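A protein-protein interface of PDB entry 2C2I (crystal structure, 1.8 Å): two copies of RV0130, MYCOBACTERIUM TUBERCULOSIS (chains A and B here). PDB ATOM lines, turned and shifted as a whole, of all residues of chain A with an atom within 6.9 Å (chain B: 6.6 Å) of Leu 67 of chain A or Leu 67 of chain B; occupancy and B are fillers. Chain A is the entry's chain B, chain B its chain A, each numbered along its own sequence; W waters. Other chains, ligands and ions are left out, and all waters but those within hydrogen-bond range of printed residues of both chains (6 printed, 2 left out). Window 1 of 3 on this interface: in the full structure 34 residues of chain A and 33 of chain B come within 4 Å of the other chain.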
ATOM      1  N   HIS A  62       0.246   5.930  10.257  1.00  0.00           N
ATOM      2  CA  HIS A  62       1.616   5.728  10.654  1.00  0.00           C
ATOM      3  C   HIS A  62       2.309   5.021   9.497  1.00  0.00           C
ATOM      4  O   HIS A  62       1.785   4.040   8.975  1.00  0.00           O
ATOM      5  CB  HIS A  62       1.711   4.746  11.837  1.00  0.00           C
ATOM      6  CG  HIS A  62       1.020   5.190  13.095  1.00  0.00           C
ATOM      7  ND1 HIS A  62      -0.346   5.080  13.284  1.00  0.00           N
ATOM      8  CD2 HIS A  62       1.529   5.649  14.263  1.00  0.00           C
ATOM      9  CE1 HIS A  62      -0.652   5.512  14.498  1.00  0.00           C
ATOM     10  NE2 HIS A  62       0.470   5.847  15.120  1.00  0.00           N
ATOM     11  N   GLY A  63       3.499   5.480   9.129  1.00  0.00           N
ATOM     12  CA  GLY A  63       4.257   4.762   8.086  1.00  0.00           C
ATOM     13  C   GLY A  63       4.468   3.315   8.456  1.00  0.00           C
ATOM     14  O   GLY A  63       4.357   2.419   7.601  1.00  0.00           O
ATOM     15  N   PHE A  64       4.763   3.060   9.735  1.00  0.00           N
ATOM     16  CA  PHE A  64       4.950   1.686  10.197  1.00  0.00           C
ATOM     17  C   PHE A  64       3.654   0.858  10.071  1.00  0.00           C
ATOM     18  O   PHE A  64       3.707  -0.373   9.983  1.00  0.00           O
ATOM     19  CB  PHE A  64       5.450   1.635  11.642  1.00  0.00           C
ATOM     20  CG  PHE A  64       6.928   1.935  11.800  1.00  0.00           C
ATOM     21  CD1 PHE A  64       7.882   1.236  11.053  1.00  0.00           C
ATOM     22  CD2 PHE A  64       7.339   2.889  12.726  1.00  0.00           C
ATOM     23  CE1 PHE A  64       9.260   1.491  11.222  1.00  0.00           C
ATOM     24  CE2 PHE A  64       8.719   3.174  12.908  1.00  0.00           C
ATOM     25  CZ  PHE A  64       9.663   2.474  12.155  1.00  0.00           C
ATOM     26  N   MET A  65       2.502   1.517  10.070  1.00  0.00           N
ATOM     27  CA  MET A  65       1.283   0.752   9.824  1.00  0.00           C
ATOM     28  C   MET A  65       1.160   0.426   8.353  1.00  0.00           C
ATOM     29  O   MET A  65       0.903  -0.707   8.015  1.00  0.00           O
ATOM     30  CB  MET A  65       0.006   1.438  10.301  1.00  0.00           C
ATOM     31  CG  MET A  65      -1.210   0.503  10.081  1.00  0.00           C
ATOM     32  SD  MET A  65      -2.908   1.177  10.799  1.00  0.00           S
ATOM     33  CE  MET A  65      -2.768   2.411  10.440  1.00  0.00           C
ATOM     34  N   THR A  66       1.356   1.406   7.462  1.00  0.00           N
ATOM     35  CA  THR A  66       1.279   1.093   6.036  1.00  0.00           C
ATOM     36  C   THR A  66       2.215  -0.096   5.676  1.00  0.00           C
ATOM     37  O   THR A  66       1.853  -1.038   4.926  1.00  0.00           O
ATOM     38  CB  THR A  66       1.606   2.345   5.215  1.00  0.00           C
ATOM     39  OG1 THR A  66       0.615   3.363   5.505  1.00  0.00           O
ATOM     40  CG2 THR A  66       1.597   2.021   3.739  1.00  0.00           C
ATOM     41  N   LEU A  67       3.421  -0.061   6.229  1.00  0.00           N
ATOM     42  CA  LEU A  67       4.385  -1.159   6.044  1.00  0.00           C
ATOM     43  C   LEU A  67       3.853  -2.489   6.577  1.00  0.00           C
ATOM     44  O   LEU A  67       3.961  -3.518   5.915  1.00  0.00           O
ATOM     45  CB  LEU A  67       5.706  -0.823   6.736  1.00  0.00           C
ATOM     46  CG  LEU A  67       6.828  -1.851   6.559  1.00  0.00           C
ATOM     47  CD1 LEU A  67       7.164  -2.017   5.063  1.00  0.00           C
ATOM     48  CD2 LEU A  67       8.062  -1.441   7.408  1.00  0.00           C
ATOM     49  N   ALA A  68       3.244  -2.435   7.765  1.00  0.00           N
ATOM     50  CA  ALA A  68       2.668  -3.604   8.450  1.00  0.00           C
ATOM     51  C   ALA A  68       1.418  -4.169   7.763  1.00  0.00           C
ATOM     52  O   ALA A  68       0.935  -5.240   8.136  1.00  0.00           O
ATOM     53  CB  ALA A  68       2.331  -3.233   9.879  1.00  0.00           C
ATOM     54  N   LEU A  69       0.870  -3.428   6.791  1.00  0.00           N
ATOM     55  CA  LEU A  69      -0.218  -3.953   5.964  1.00  0.00           C
ATOM     56  C   LEU A  69       0.271  -4.912   4.876  1.00  0.00           C
ATOM     57  O   LEU A  69      -0.551  -5.533   4.183  1.00  0.00           O
ATOM     58  CB  LEU A  69      -1.008  -2.809   5.315  1.00  0.00           C
ATOM     59  CG  LEU A  69      -1.867  -1.894   6.182  1.00  0.00           C
ATOM     60  CD1 LEU A  69      -2.576  -0.888   5.262  1.00  0.00           C
ATOM     61  CD2 LEU A  69      -2.883  -2.725   6.989  1.00  0.00           C
ATOM     62  N   LEU A  70       1.589  -5.031   4.701  1.00  0.00           N
ATOM     63  CA  LEU A  70       2.122  -5.936   3.664  1.00  0.00           C
ATOM     64  C   LEU A  70       1.558  -7.371   3.766  1.00  0.00           C
ATOM     65  O   LEU A  70       1.062  -7.887   2.764  1.00  0.00           O
ATOM     66  CB  LEU A  70       3.665  -5.907   3.579  1.00  0.00           C
ATOM     67  CG  LEU A  70       4.264  -5.041   2.476  1.00  0.00           C
ATOM     68  CD1 LEU A  70       3.796  -3.556   2.549  1.00  0.00           C
ATOM     69  CD2 LEU A  70       5.796  -5.132   2.569  1.00  0.00           C
ATOM     70  N   PRO A  71       1.608  -8.000   4.968  1.00  0.00           N
ATOM     71  CA  PRO A  71       0.992  -9.337   5.097  1.00  0.00           C
ATOM     72  C   PRO A  71      -0.484  -9.380   4.629  1.00  0.00           C
ATOM     73  O   PRO A  71      -0.826 -10.185   3.757  1.00  0.00           O
ATOM     74  CB  PRO A  71       1.149  -9.660   6.593  1.00  0.00           C
ATOM     75  CG  PRO A  71       2.454  -8.921   6.946  1.00  0.00           C
ATOM     76  CD  PRO A  71       2.293  -7.604   6.219  1.00  0.00           C
ATOM     77  N   ASN A  88       8.137 -12.881   9.629  1.00  0.00           N
ATOM     78  CA  ASN A  88       8.872 -11.715   9.158  1.00  0.00           C
ATOM     79  C   ASN A  88      10.370 -11.868   9.481  1.00  0.00           C
ATOM     80  O   ASN A  88      10.770 -11.949  10.653  1.00  0.00           O
ATOM     81  CB  ASN A  88       8.269 -10.477   9.846  1.00  0.00           C
ATOM     82  CG  ASN A  88       8.738  -9.175   9.246  1.00  0.00           C
ATOM     83  OD1 ASN A  88       9.753  -9.115   8.541  1.00  0.00           O
ATOM     84  ND2 ASN A  88       7.993  -8.120   9.523  1.00  0.00           N
ATOM     85  N   LEU A  91      13.495  -6.376   6.682  1.00  0.00           N
ATOM     86  CA  LEU A  91      13.280  -5.471   5.555  1.00  0.00           C
ATOM     87  C   LEU A  91      14.655  -5.094   5.009  1.00  0.00           C
ATOM     88  O   LEU A  91      15.623  -5.044   5.768  1.00  0.00           O
ATOM     89  CB  LEU A  91      12.555  -4.191   6.032  1.00  0.00           C
ATOM     90  CG  LEU A  91      11.088  -4.240   6.517  1.00  0.00           C
ATOM     91  CD1 LEU A  91      10.221  -4.894   5.432  1.00  0.00           C
ATOM     92  CD2 LEU A  91      10.913  -4.909   7.891  1.00  0.00           C
ATOM     93  N   VAL A  94      13.239   0.537   2.559  1.00  0.00           N
ATOM     94  CA  VAL A  94      11.834   0.948   2.610  1.00  0.00           C
ATOM     95  C   VAL A  94      11.771   2.475   2.549  1.00  0.00           C
ATOM     96  O   VAL A  94      12.505   3.136   3.252  1.00  0.00           O
ATOM     97  CB  VAL A  94      11.104   0.472   3.885  1.00  0.00           C
ATOM     98  CG1 VAL A  94       9.629   0.955   3.872  1.00  0.00           C
ATOM     99  CG2 VAL A  94      11.142  -1.079   4.003  1.00  0.00           C
ATOM    100  N   PHE A  96       8.757   5.896   2.188  1.00  0.00           N
ATOM    101  CA  PHE A  96       7.348   6.281   2.295  1.00  0.00           C
ATOM    102  C   PHE A  96       7.201   7.640   1.585  1.00  0.00           C
ATOM    103  O   PHE A  96       7.178   8.674   2.253  1.00  0.00           O
ATOM    104  CB  PHE A  96       6.964   6.429   3.782  1.00  0.00           C
ATOM    105  CG  PHE A  96       7.053   5.149   4.582  1.00  0.00           C
ATOM    106  CD1 PHE A  96       6.137   4.116   4.367  1.00  0.00           C
ATOM    107  CD2 PHE A  96       8.044   4.985   5.556  1.00  0.00           C
ATOM    108  CE1 PHE A  96       6.219   2.923   5.107  1.00  0.00           C
ATOM    109  CE2 PHE A  96       8.130   3.796   6.305  1.00  0.00           C
ATOM    110  CZ  PHE A  96       7.195   2.786   6.084  1.00  0.00           C
ATOM    111  N   VAL A 131       3.064   0.171  -2.590  1.00  0.00           N
ATOM    112  CA  VAL A 131       1.733   0.485  -2.077  1.00  0.00           C
ATOM    113  C   VAL A 131       1.374   1.838  -2.678  1.00  0.00           C
ATOM    114  O   VAL A 131       2.092   2.838  -2.470  1.00  0.00           O
ATOM    115  CB  VAL A 131       1.714   0.559  -0.541  1.00  0.00           C
ATOM    116  CG1 VAL A 131       0.296   0.939  -0.069  1.00  0.00           C
ATOM    117  CG2 VAL A 131       2.151  -0.803   0.048  1.00  0.00           C
ATOM    118  N   CYS A 141       4.397   3.761  -0.354  1.00  0.00           N
ATOM    119  CA  CYS A 141       5.487   2.939   0.160  1.00  0.00           C
ATOM    120  C   CYS A 141       6.125   2.154  -1.003  1.00  0.00           C
ATOM    121  O   CYS A 141       5.436   1.662  -1.891  1.00  0.00           O
ATOM    122  CB  CYS A 141       4.952   1.990   1.253  1.00  0.00           C
ATOM    123  SG  CYS A 141       6.213   0.864   2.027  1.00  0.00           S
ATOM    124  N   VAL A 142       7.452   2.067  -0.984  1.00  0.00           N
ATOM    125  CA  VAL A 142       8.168   1.114  -1.846  1.00  0.00           C
ATOM    126  C   VAL A 142       9.055   0.338  -0.887  1.00  0.00           C
ATOM    127  O   VAL A 142       9.897   0.918  -0.208  1.00  0.00           O
ATOM    128  CB  VAL A 142       8.988   1.811  -2.953  1.00  0.00           C
ATOM    129  CG1 VAL A 142       9.771   0.781  -3.746  1.00  0.00           C
ATOM    130  CG2 VAL A 142       8.053   2.604  -3.882  1.00  0.00           C
ATOM    131  N   ALA A 143       8.853  -0.978  -0.811  1.00  0.00           N
ATOM    132  CA  ALA A 143       9.546  -1.756   0.227  1.00  0.00           C
ATOM    133  C   ALA A 143      10.064  -3.081  -0.287  1.00  0.00           C
ATOM    134  O   ALA A 143       9.418  -3.726  -1.105  1.00  0.00           O
ATOM    135  CB  ALA A 143       8.597  -2.013   1.368  1.00  0.00           C
ATOM    136  N   GLU A 144      11.228  -3.491   0.214  1.00  0.00           N
ATOM    137  CA  GLU A 144      11.707  -4.870  -0.012  1.00  0.00           C
ATOM    138  C   GLU A 144      11.680  -5.569   1.357  1.00  0.00           C
ATOM    139  O   GLU A 144      12.262  -5.087   2.332  1.00  0.00           O
ATOM    140  CB  GLU A 144      13.113  -4.900  -0.616  1.00  0.00           C
ATOM    141  CG  GLU A 144      13.613  -6.319  -0.937  1.00  0.00           C
ATOM    142  CD  GLU A 144      14.896  -6.294  -1.726  1.00  0.00           C
ATOM    143  OE1 GLU A 144      14.819  -6.128  -2.962  1.00  0.00           O
ATOM    144  OE2 GLU A 144      15.976  -6.422  -1.108  1.00  0.00           O
ATOM    145  N   SER A 145      10.960  -6.681   1.409  1.00  0.00           N
ATOM    146  CA  SER A 145      10.719  -7.386   2.671  1.00  0.00           C
ATOM    147  C   SER A 145      11.196  -8.813   2.529  1.00  0.00           C
ATOM    148  O   SER A 145      11.397  -9.312   1.419  1.00  0.00           O
ATOM    149  CB  SER A 145       9.226  -7.352   3.031  1.00  0.00           C
ATOM    150  OG  SER A 145       8.451  -7.929   1.970  1.00  0.00           O
ATOM    151  N   HIS B  62       4.340  -9.752  16.509  1.00  0.00           N
ATOM    152  CA  HIS B  62       4.596  -9.516  15.090  1.00  0.00           C
ATOM    153  C   HIS B  62       5.929  -8.770  15.002  1.00  0.00           C
ATOM    154  O   HIS B  62       6.141  -7.831  15.757  1.00  0.00           O
ATOM    155  CB  HIS B  62       3.533  -8.584  14.501  1.00  0.00           C
ATOM    156  CG  HIS B  62       2.129  -9.096  14.588  1.00  0.00           C
ATOM    157  ND1 HIS B  62       1.405  -9.098  15.762  1.00  0.00           N
ATOM    158  CD2 HIS B  62       1.285  -9.537  13.622  1.00  0.00           C
ATOM    159  CE1 HIS B  62       0.192  -9.570  15.526  1.00  0.00           C
ATOM    160  NE2 HIS B  62       0.096  -9.852  14.236  1.00  0.00           N
ATOM    161  N   GLY B  63       6.821  -9.189  14.118  1.00  0.00           N
ATOM    162  CA  GLY B  63       8.042  -8.392  13.843  1.00  0.00           C
ATOM    163  C   GLY B  63       7.704  -6.956  13.466  1.00  0.00           C
ATOM    164  O   GLY B  63       8.432  -6.003  13.856  1.00  0.00           O
ATOM    165  N   PHE B  64       6.598  -6.764  12.749  1.00  0.00           N
ATOM    166  CA  PHE B  64       6.247  -5.411  12.331  1.00  0.00           C
ATOM    167  C   PHE B  64       5.851  -4.588  13.538  1.00  0.00           C
ATOM    168  O   PHE B  64       5.952  -3.372  13.503  1.00  0.00           O
ATOM    169  CB  PHE B  64       5.136  -5.392  11.274  1.00  0.00           C
ATOM    170  CG  PHE B  64       5.612  -5.643   9.863  1.00  0.00           C
ATOM    171  CD1 PHE B  64       6.619  -4.845   9.279  1.00  0.00           C
ATOM    172  CD2 PHE B  64       5.040  -6.661   9.107  1.00  0.00           C
ATOM    173  CE1 PHE B  64       7.023  -5.075   7.965  1.00  0.00           C
ATOM    174  CE2 PHE B  64       5.433  -6.879   7.764  1.00  0.00           C
ATOM    175  CZ  PHE B  64       6.428  -6.112   7.202  1.00  0.00           C
ATOM    176  N   MET B  65       5.392  -5.254  14.607  1.00  0.00           N
ATOM    177  CA  MET B  65       5.043  -4.504  15.800  1.00  0.00           C
ATOM    178  C   MET B  65       6.295  -4.094  16.560  1.00  0.00           C
ATOM    179  O   MET B  65       6.416  -2.946  16.936  1.00  0.00           O
ATOM    180  CB  MET B  65       4.128  -5.278  16.740  1.00  0.00           C
ATOM    181  CG  MET B  65       3.797  -4.424  17.975  1.00  0.00           C
ATOM    182  SD  MET B  65       2.429  -5.216  19.092  1.00  0.00           S
ATOM    183  CE  MET B  65       2.971  -6.523  19.092  1.00  0.00           C
ATOM    184  N   THR B  66       7.207  -5.034  16.791  1.00  0.00           N
ATOM    185  CA  THR B  66       8.461  -4.717  17.507  1.00  0.00           C
ATOM    186  C   THR B  66       9.188  -3.552  16.798  1.00  0.00           C
ATOM    187  O   THR B  66       9.645  -2.591  17.427  1.00  0.00           O
ATOM    188  CB  THR B  66       9.357  -5.970  17.612  1.00  0.00           C
ATOM    189  OG1 THR B  66       8.639  -6.996  18.332  1.00  0.00           O
ATOM    190  CG2 THR B  66      10.637  -5.674  18.385  1.00  0.00           C
ATOM    191  N   LEU B  67       9.251  -3.636  15.479  1.00  0.00           N
ATOM    192  CA  LEU B  67       9.849  -2.554  14.674  1.00  0.00           C
ATOM    193  C   LEU B  67       9.123  -1.238  14.950  1.00  0.00           C
ATOM    194  O   LEU B  67       9.760  -0.213  15.127  1.00  0.00           O
ATOM    195  CB  LEU B  67       9.792  -2.891  13.170  1.00  0.00           C
ATOM    196  CG  LEU B  67      10.265  -1.769  12.222  1.00  0.00           C
ATOM    197  CD1 LEU B  67      11.739  -1.449  12.446  1.00  0.00           C
ATOM    198  CD2 LEU B  67      10.012  -2.172  10.767  1.00  0.00           C
ATOM    199  N   ALA B  68       7.788  -1.286  14.984  1.00  0.00           N
ATOM    200  CA  ALA B  68       6.931  -0.115  15.218  1.00  0.00           C
ATOM    201  C   ALA B  68       6.973   0.422  16.655  1.00  0.00           C
ATOM    202  O   ALA B  68       6.398   1.481  16.938  1.00  0.00           O
ATOM    203  CB  ALA B  68       5.477  -0.427  14.795  1.00  0.00           C
ATOM    204  N   LEU B  69       7.638  -0.301  17.560  1.00  0.00           N
ATOM    205  CA  LEU B  69       7.928   0.266  18.877  1.00  0.00           C
ATOM    206  C   LEU B  69       9.039   1.345  18.860  1.00  0.00           C
ATOM    207  O   LEU B  69       9.248   2.023  19.861  1.00  0.00           O
ATOM    208  CB  LEU B  69       8.272  -0.825  19.902  1.00  0.00           C
ATOM    209  CG  LEU B  69       7.263  -1.943  20.173  1.00  0.00           C
ATOM    210  CD1 LEU B  69       7.878  -2.989  21.119  1.00  0.00           C
ATOM    211  CD2 LEU B  69       5.964  -1.372  20.758  1.00  0.00           C
ATOM    212  N   LEU B  70       9.720   1.526  17.731  1.00  0.00           N
ATOM    213  CA  LEU B  70      10.842   2.476  17.680  1.00  0.00           C
ATOM    214  C   LEU B  70      10.483   3.903  18.120  1.00  0.00           C
ATOM    215  O   LEU B  70      11.207   4.503  18.926  1.00  0.00           O
ATOM    216  CB  LEU B  70      11.549   2.459  16.306  1.00  0.00           C
ATOM    217  CG  LEU B  70      12.855   1.672  16.229  1.00  0.00           C
ATOM    218  CD1 LEU B  70      12.666   0.230  16.772  1.00  0.00           C
ATOM    219  CD2 LEU B  70      13.376   1.713  14.777  1.00  0.00           C
ATOM    220  N   PRO B  71       9.389   4.473  17.579  1.00  0.00           N
ATOM    221  CA  PRO B  71       8.981   5.807  18.056  1.00  0.00           C
ATOM    222  C   PRO B  71       8.771   5.928  19.579  1.00  0.00           C
ATOM    223  O   PRO B  71       9.326   6.842  20.199  1.00  0.00           O
ATOM    224  CB  PRO B  71       7.687   6.084  17.268  1.00  0.00           C
ATOM    225  CG  PRO B  71       7.898   5.270  15.951  1.00  0.00           C
ATOM    226  CD  PRO B  71       8.541   4.002  16.458  1.00  0.00           C
ATOM    227  N   ASN B  88       7.850   9.236   9.649  1.00  0.00           N
ATOM    228  CA  ASN B  88       8.675   8.099   9.266  1.00  0.00           C
ATOM    229  C   ASN B  88       8.929   8.170   7.753  1.00  0.00           C
ATOM    230  O   ASN B  88       7.991   8.101   6.958  1.00  0.00           O
ATOM    231  CB  ASN B  88       7.911   6.836   9.694  1.00  0.00           C
ATOM    232  CG  ASN B  88       8.642   5.552   9.395  1.00  0.00           C
ATOM    233  OD1 ASN B  88       9.697   5.523   8.733  1.00  0.00           O
ATOM    234  ND2 ASN B  88       8.062   4.444   9.890  1.00  0.00           N
ATOM    235  N   LEU B  91      13.299   3.075   6.036  1.00  0.00           N
ATOM    236  CA  LEU B  91      14.239   2.183   6.732  1.00  0.00           C
ATOM    237  C   LEU B  91      15.286   1.784   5.706  1.00  0.00           C
ATOM    238  O   LEU B  91      14.966   1.631   4.533  1.00  0.00           O
ATOM    239  CB  LEU B  91      13.512   0.910   7.190  1.00  0.00           C
ATOM    240  CG  LEU B  91      12.288   1.191   8.082  1.00  0.00           C
ATOM    241  CD1 LEU B  91      11.297   0.085   7.972  1.00  0.00           C
ATOM    242  CD2 LEU B  91      12.760   1.432   9.520  1.00  0.00           C
ATOM    243  N   LYS B  93      17.557  -0.919   6.606  1.00  0.00           N
ATOM    244  CA  LYS B  93      17.687  -2.378   6.859  1.00  0.00           C
ATOM    245  C   LYS B  93      17.046  -2.697   8.188  1.00  0.00           C
ATOM    246  O   LYS B  93      17.123  -1.895   9.128  1.00  0.00           O
ATOM    247  CB  LYS B  93      19.151  -2.800   6.920  1.00  0.00           C
ATOM    248  CG  LYS B  93      19.360  -4.315   6.822  1.00  0.00           C
ATOM    249  CD  LYS B  93      20.842  -4.656   6.843  1.00  0.00           C
ATOM    250  CE  LYS B  93      21.019  -6.167   6.975  1.00  0.00           C
ATOM    251  NZ  LYS B  93      22.449  -6.565   6.849  1.00  0.00           N
ATOM    252  N   VAL B  94      16.407  -3.862   8.270  1.00  0.00           N
ATOM    253  CA  VAL B  94      15.822  -4.317   9.540  1.00  0.00           C
ATOM    254  C   VAL B  94      15.989  -5.835   9.579  1.00  0.00           C
ATOM    255  O   VAL B  94      15.725  -6.508   8.581  1.00  0.00           O
ATOM    256  CB  VAL B  94      14.279  -4.018   9.651  1.00  0.00           C
ATOM    257  CG1 VAL B  94      13.744  -4.610  10.940  1.00  0.00           C
ATOM    258  CG2 VAL B  94      13.950  -2.454   9.541  1.00  0.00           C
ATOM    259  N   PHE B  96      15.308  -9.334  12.442  1.00  0.00           N
ATOM    260  CA  PHE B  96      14.636  -9.751  13.673  1.00  0.00           C
ATOM    261  C   PHE B  96      15.288 -11.042  14.157  1.00  0.00           C
ATOM    262  O   PHE B  96      14.713 -12.142  13.980  1.00  0.00           O
ATOM    263  CB  PHE B  96      13.139 -10.004  13.418  1.00  0.00           C
ATOM    264  CG  PHE B  96      12.384  -8.792  12.920  1.00  0.00           C
ATOM    265  CD1 PHE B  96      12.103  -7.738  13.775  1.00  0.00           C
ATOM    266  CD2 PHE B  96      11.969  -8.713  11.596  1.00  0.00           C
ATOM    267  CE1 PHE B  96      11.394  -6.616  13.331  1.00  0.00           C
ATOM    268  CE2 PHE B  96      11.252  -7.589  11.132  1.00  0.00           C
ATOM    269  CZ  PHE B  96      10.972  -6.545  11.990  1.00  0.00           C
ATOM    270  N   VAL B 131      17.039  -3.474  19.471  1.00  0.00           N
ATOM    271  CA  VAL B 131      16.047  -3.792  20.480  1.00  0.00           C
ATOM    272  C   VAL B 131      16.437  -5.147  21.078  1.00  0.00           C
ATOM    273  O   VAL B 131      16.474  -6.161  20.366  1.00  0.00           O
ATOM    274  CB  VAL B 131      14.599  -3.865  19.891  1.00  0.00           C
ATOM    275  CG1 VAL B 131      13.571  -4.066  21.000  1.00  0.00           C
ATOM    276  CG2 VAL B 131      14.251  -2.592  19.128  1.00  0.00           C
ATOM    277  N   CYS B 141      15.409  -6.974  17.413  1.00  0.00           N
ATOM    278  CA  CYS B 141      15.329  -6.166  16.204  1.00  0.00           C
ATOM    279  C   CYS B 141      16.590  -5.328  16.095  1.00  0.00           C
ATOM    280  O   CYS B 141      17.041  -4.760  17.088  1.00  0.00           O
ATOM    281  CB  CYS B 141      14.101  -5.265  16.292  1.00  0.00           C
ATOM    282  SG  CYS B 141      13.858  -4.230  14.810  1.00  0.00           S
ATOM    283  N   VAL B 142      17.158  -5.275  14.890  1.00  0.00           N
ATOM    284  CA  VAL B 142      18.260  -4.374  14.564  1.00  0.00           C
ATOM    285  C   VAL B 142      17.768  -3.595  13.343  1.00  0.00           C
ATOM    286  O   VAL B 142      17.481  -4.184  12.306  1.00  0.00           O
ATOM    287  CB  VAL B 142      19.577  -5.094  14.225  1.00  0.00           C
ATOM    288  CG1 VAL B 142      20.709  -4.071  13.983  1.00  0.00           C
ATOM    289  CG2 VAL B 142      19.986  -6.098  15.325  1.00  0.00           C
ATOM    290  N   ALA B 143      17.691  -2.272  13.467  1.00  0.00           N
ATOM    291  CA  ALA B 143      17.076  -1.445  12.417  1.00  0.00           C
ATOM    292  C   ALA B 143      17.888  -0.199  12.172  1.00  0.00           C
ATOM    293  O   ALA B 143      18.417   0.381  13.104  1.00  0.00           O
ATOM    294  CB  ALA B 143      15.664  -1.037  12.818  1.00  0.00           C
ATOM    295  N   SER B 145      16.782   3.367  10.636  1.00  0.00           N
ATOM    296  CA  SER B 145      15.519   4.045  10.292  1.00  0.00           C
ATOM    297  C   SER B 145      15.798   5.513   9.961  1.00  0.00           C
ATOM    298  O   SER B 145      16.871   6.030  10.271  1.00  0.00           O
ATOM    299  CB  SER B 145      14.507   3.956  11.432  1.00  0.00           C
ATOM    300  OG  SER B 145      14.978   4.599  12.617  1.00  0.00           O
HETATM  301  O   HOH W   1       9.184 -11.410  13.001  1.00  0.00           O
HETATM  302  O   HOH W   2       6.168  -1.867  11.006  1.00  0.00           O
HETATM  303  O   HOH W   3       5.323   7.780   7.556  1.00  0.00           O
HETATM  304  O   HOH W   4      12.661 -13.638  11.680  1.00  0.00           O
HETATM  305  O   HOH W   5       6.149 -11.964  12.272  1.00  0.00           O
HETATM  306  O   HOH W   6       4.737   8.239  10.597  1.00  0.00           O
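N of Val 94 of chain B lies within hydrogen-bond range of O of Leu 91 of chain A, 2.9 Å away. N of Val 94 of chain A sits at hydrogen-bond distance from O of Leu 91 of chain B, at 2.8 Å.
Among the printed residues, merely in contact across the chains: Phe 64 of chain A with Asn 88 of chain B (3.3 Å), Asn 88 of chain A with Phe 64 of chain B (3.3 Å), Asn 88 of chain A with Phe 96 of chain B (3.4 Å), Phe 96 of chain A with Asn 88 of chain B (3.4 Å), Leu 67 of chain A with Phe 64 of chain B (3.5 Å), Leu 91 of chain A with Lys 93 of chain B (3.5 Å), Phe 64 of chain A with Leu 67 of chain B (3.6 Å), Pro 71 of chain A with Phe 64 of chain B (3.6 Å), Leu 67 of chain A with Leu 91 of chain B (3.6 Å), Phe 64 of chain A with Pro 71 of chain B (3.6 Å), Phe 64 of chain A with Ala 68 of chain B (3.8 Å), Ala 68 of chain A with Phe 64 of chain B (3.8 Å), Phe 64 of chain A with Leu 91 of chain B (3.9 Å), Leu 91 of chain A with Phe 64 of chain B (3.9 Å) and Leu 67 of chain A with Leu 67 of chain B (3.95 Å).
Leu 67 of chain A touches just these residues of chain B: Phe 64 (3.5 Å), Leu 67 (3.95 Å) and Leu 91 (3.6 Å). Of the printed residues of chain B, Leu 91 of chain A touches Phe 64 (3.9 Å), Lys 93 (3.5 Å) and Val 94 (2.9 Å). Ala 143 of chain A touches none of the printed residues of chain B. Printed residues of chain A within 4 Å of Leu 91 of chain B: Phe 64 (3.9 Å), Leu 67 (3.6 Å) and Val 94 (2.8 Å). The nearest residue of chain A that does not touch Leu 67 of chain B is Leu 91 of chain A (4.1 Å). The nearest printed residue of chain A that does not touch Phe 96 of chain B is Leu 91 of chain A (4.2 Å).
Of the 20 printed residues of chain B, 9 touch a printed residue of chain A. Of the 20 printed residues of chain A, 8 touch a printed residue of chain B. Printed residues of chain A that touch a printed residue of chain B: Phe 64, Leu 67, Ala 68, Pro 71, Asn 88, Leu 91, Val 94 and Phe 96. Hydrophobic or aromatic side chains of chain A that line the printed part of chain B: Phe 64, Leu 67, Ala 68, Pro 71, Leu 91 and Phe 96.
Phe 64 of chain A touches Pro 71 of chain B, and with the chains exchanged Pro 71 of chain A touches Phe 64 of chain B. Leu 67 of chain B touches its own counterpart, Leu 67 of chain A. Asn 88 of chain A touches Phe 96 of chain B, and with the chains exchanged Phe 96 of chain A touches Asn 88 of chain B. Positions printed for both chains: 62, 63, 64, 65, 66, 67, 68, 69, 70, 71, 88, 91, 94, 96, 131, 141, 142, 143 and 145. Of the 17 pairs that touch across the chains among the printed residues, 15 have their exchanged pair printed and touching as well.
Water W4 bridges the backbone carbonyl oxygen of Asn 88 of chain A and the backbone carbonyl oxygen of Phe 96 of chain B. Water W3 lies within hydrogen-bond range of the backbone carbonyl oxygen of Asn 88 of chain B (2.8 Å) and the backbone NH of Gly 63 of chain A (3.3 Å). Water W1 lies within hydrogen-bond range of O of Asn 88 of chain A and N of Gly 63 of chain B. Water W2 lies within hydrogen-bond range of O of Phe 64 of chain B and O of Phe 64 of chain A. Water W5 lies within hydrogen-bond range of the backbone NH (N) of Gly 63 of chain B and the backbone NH (N) of Asn 88 of chain A.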
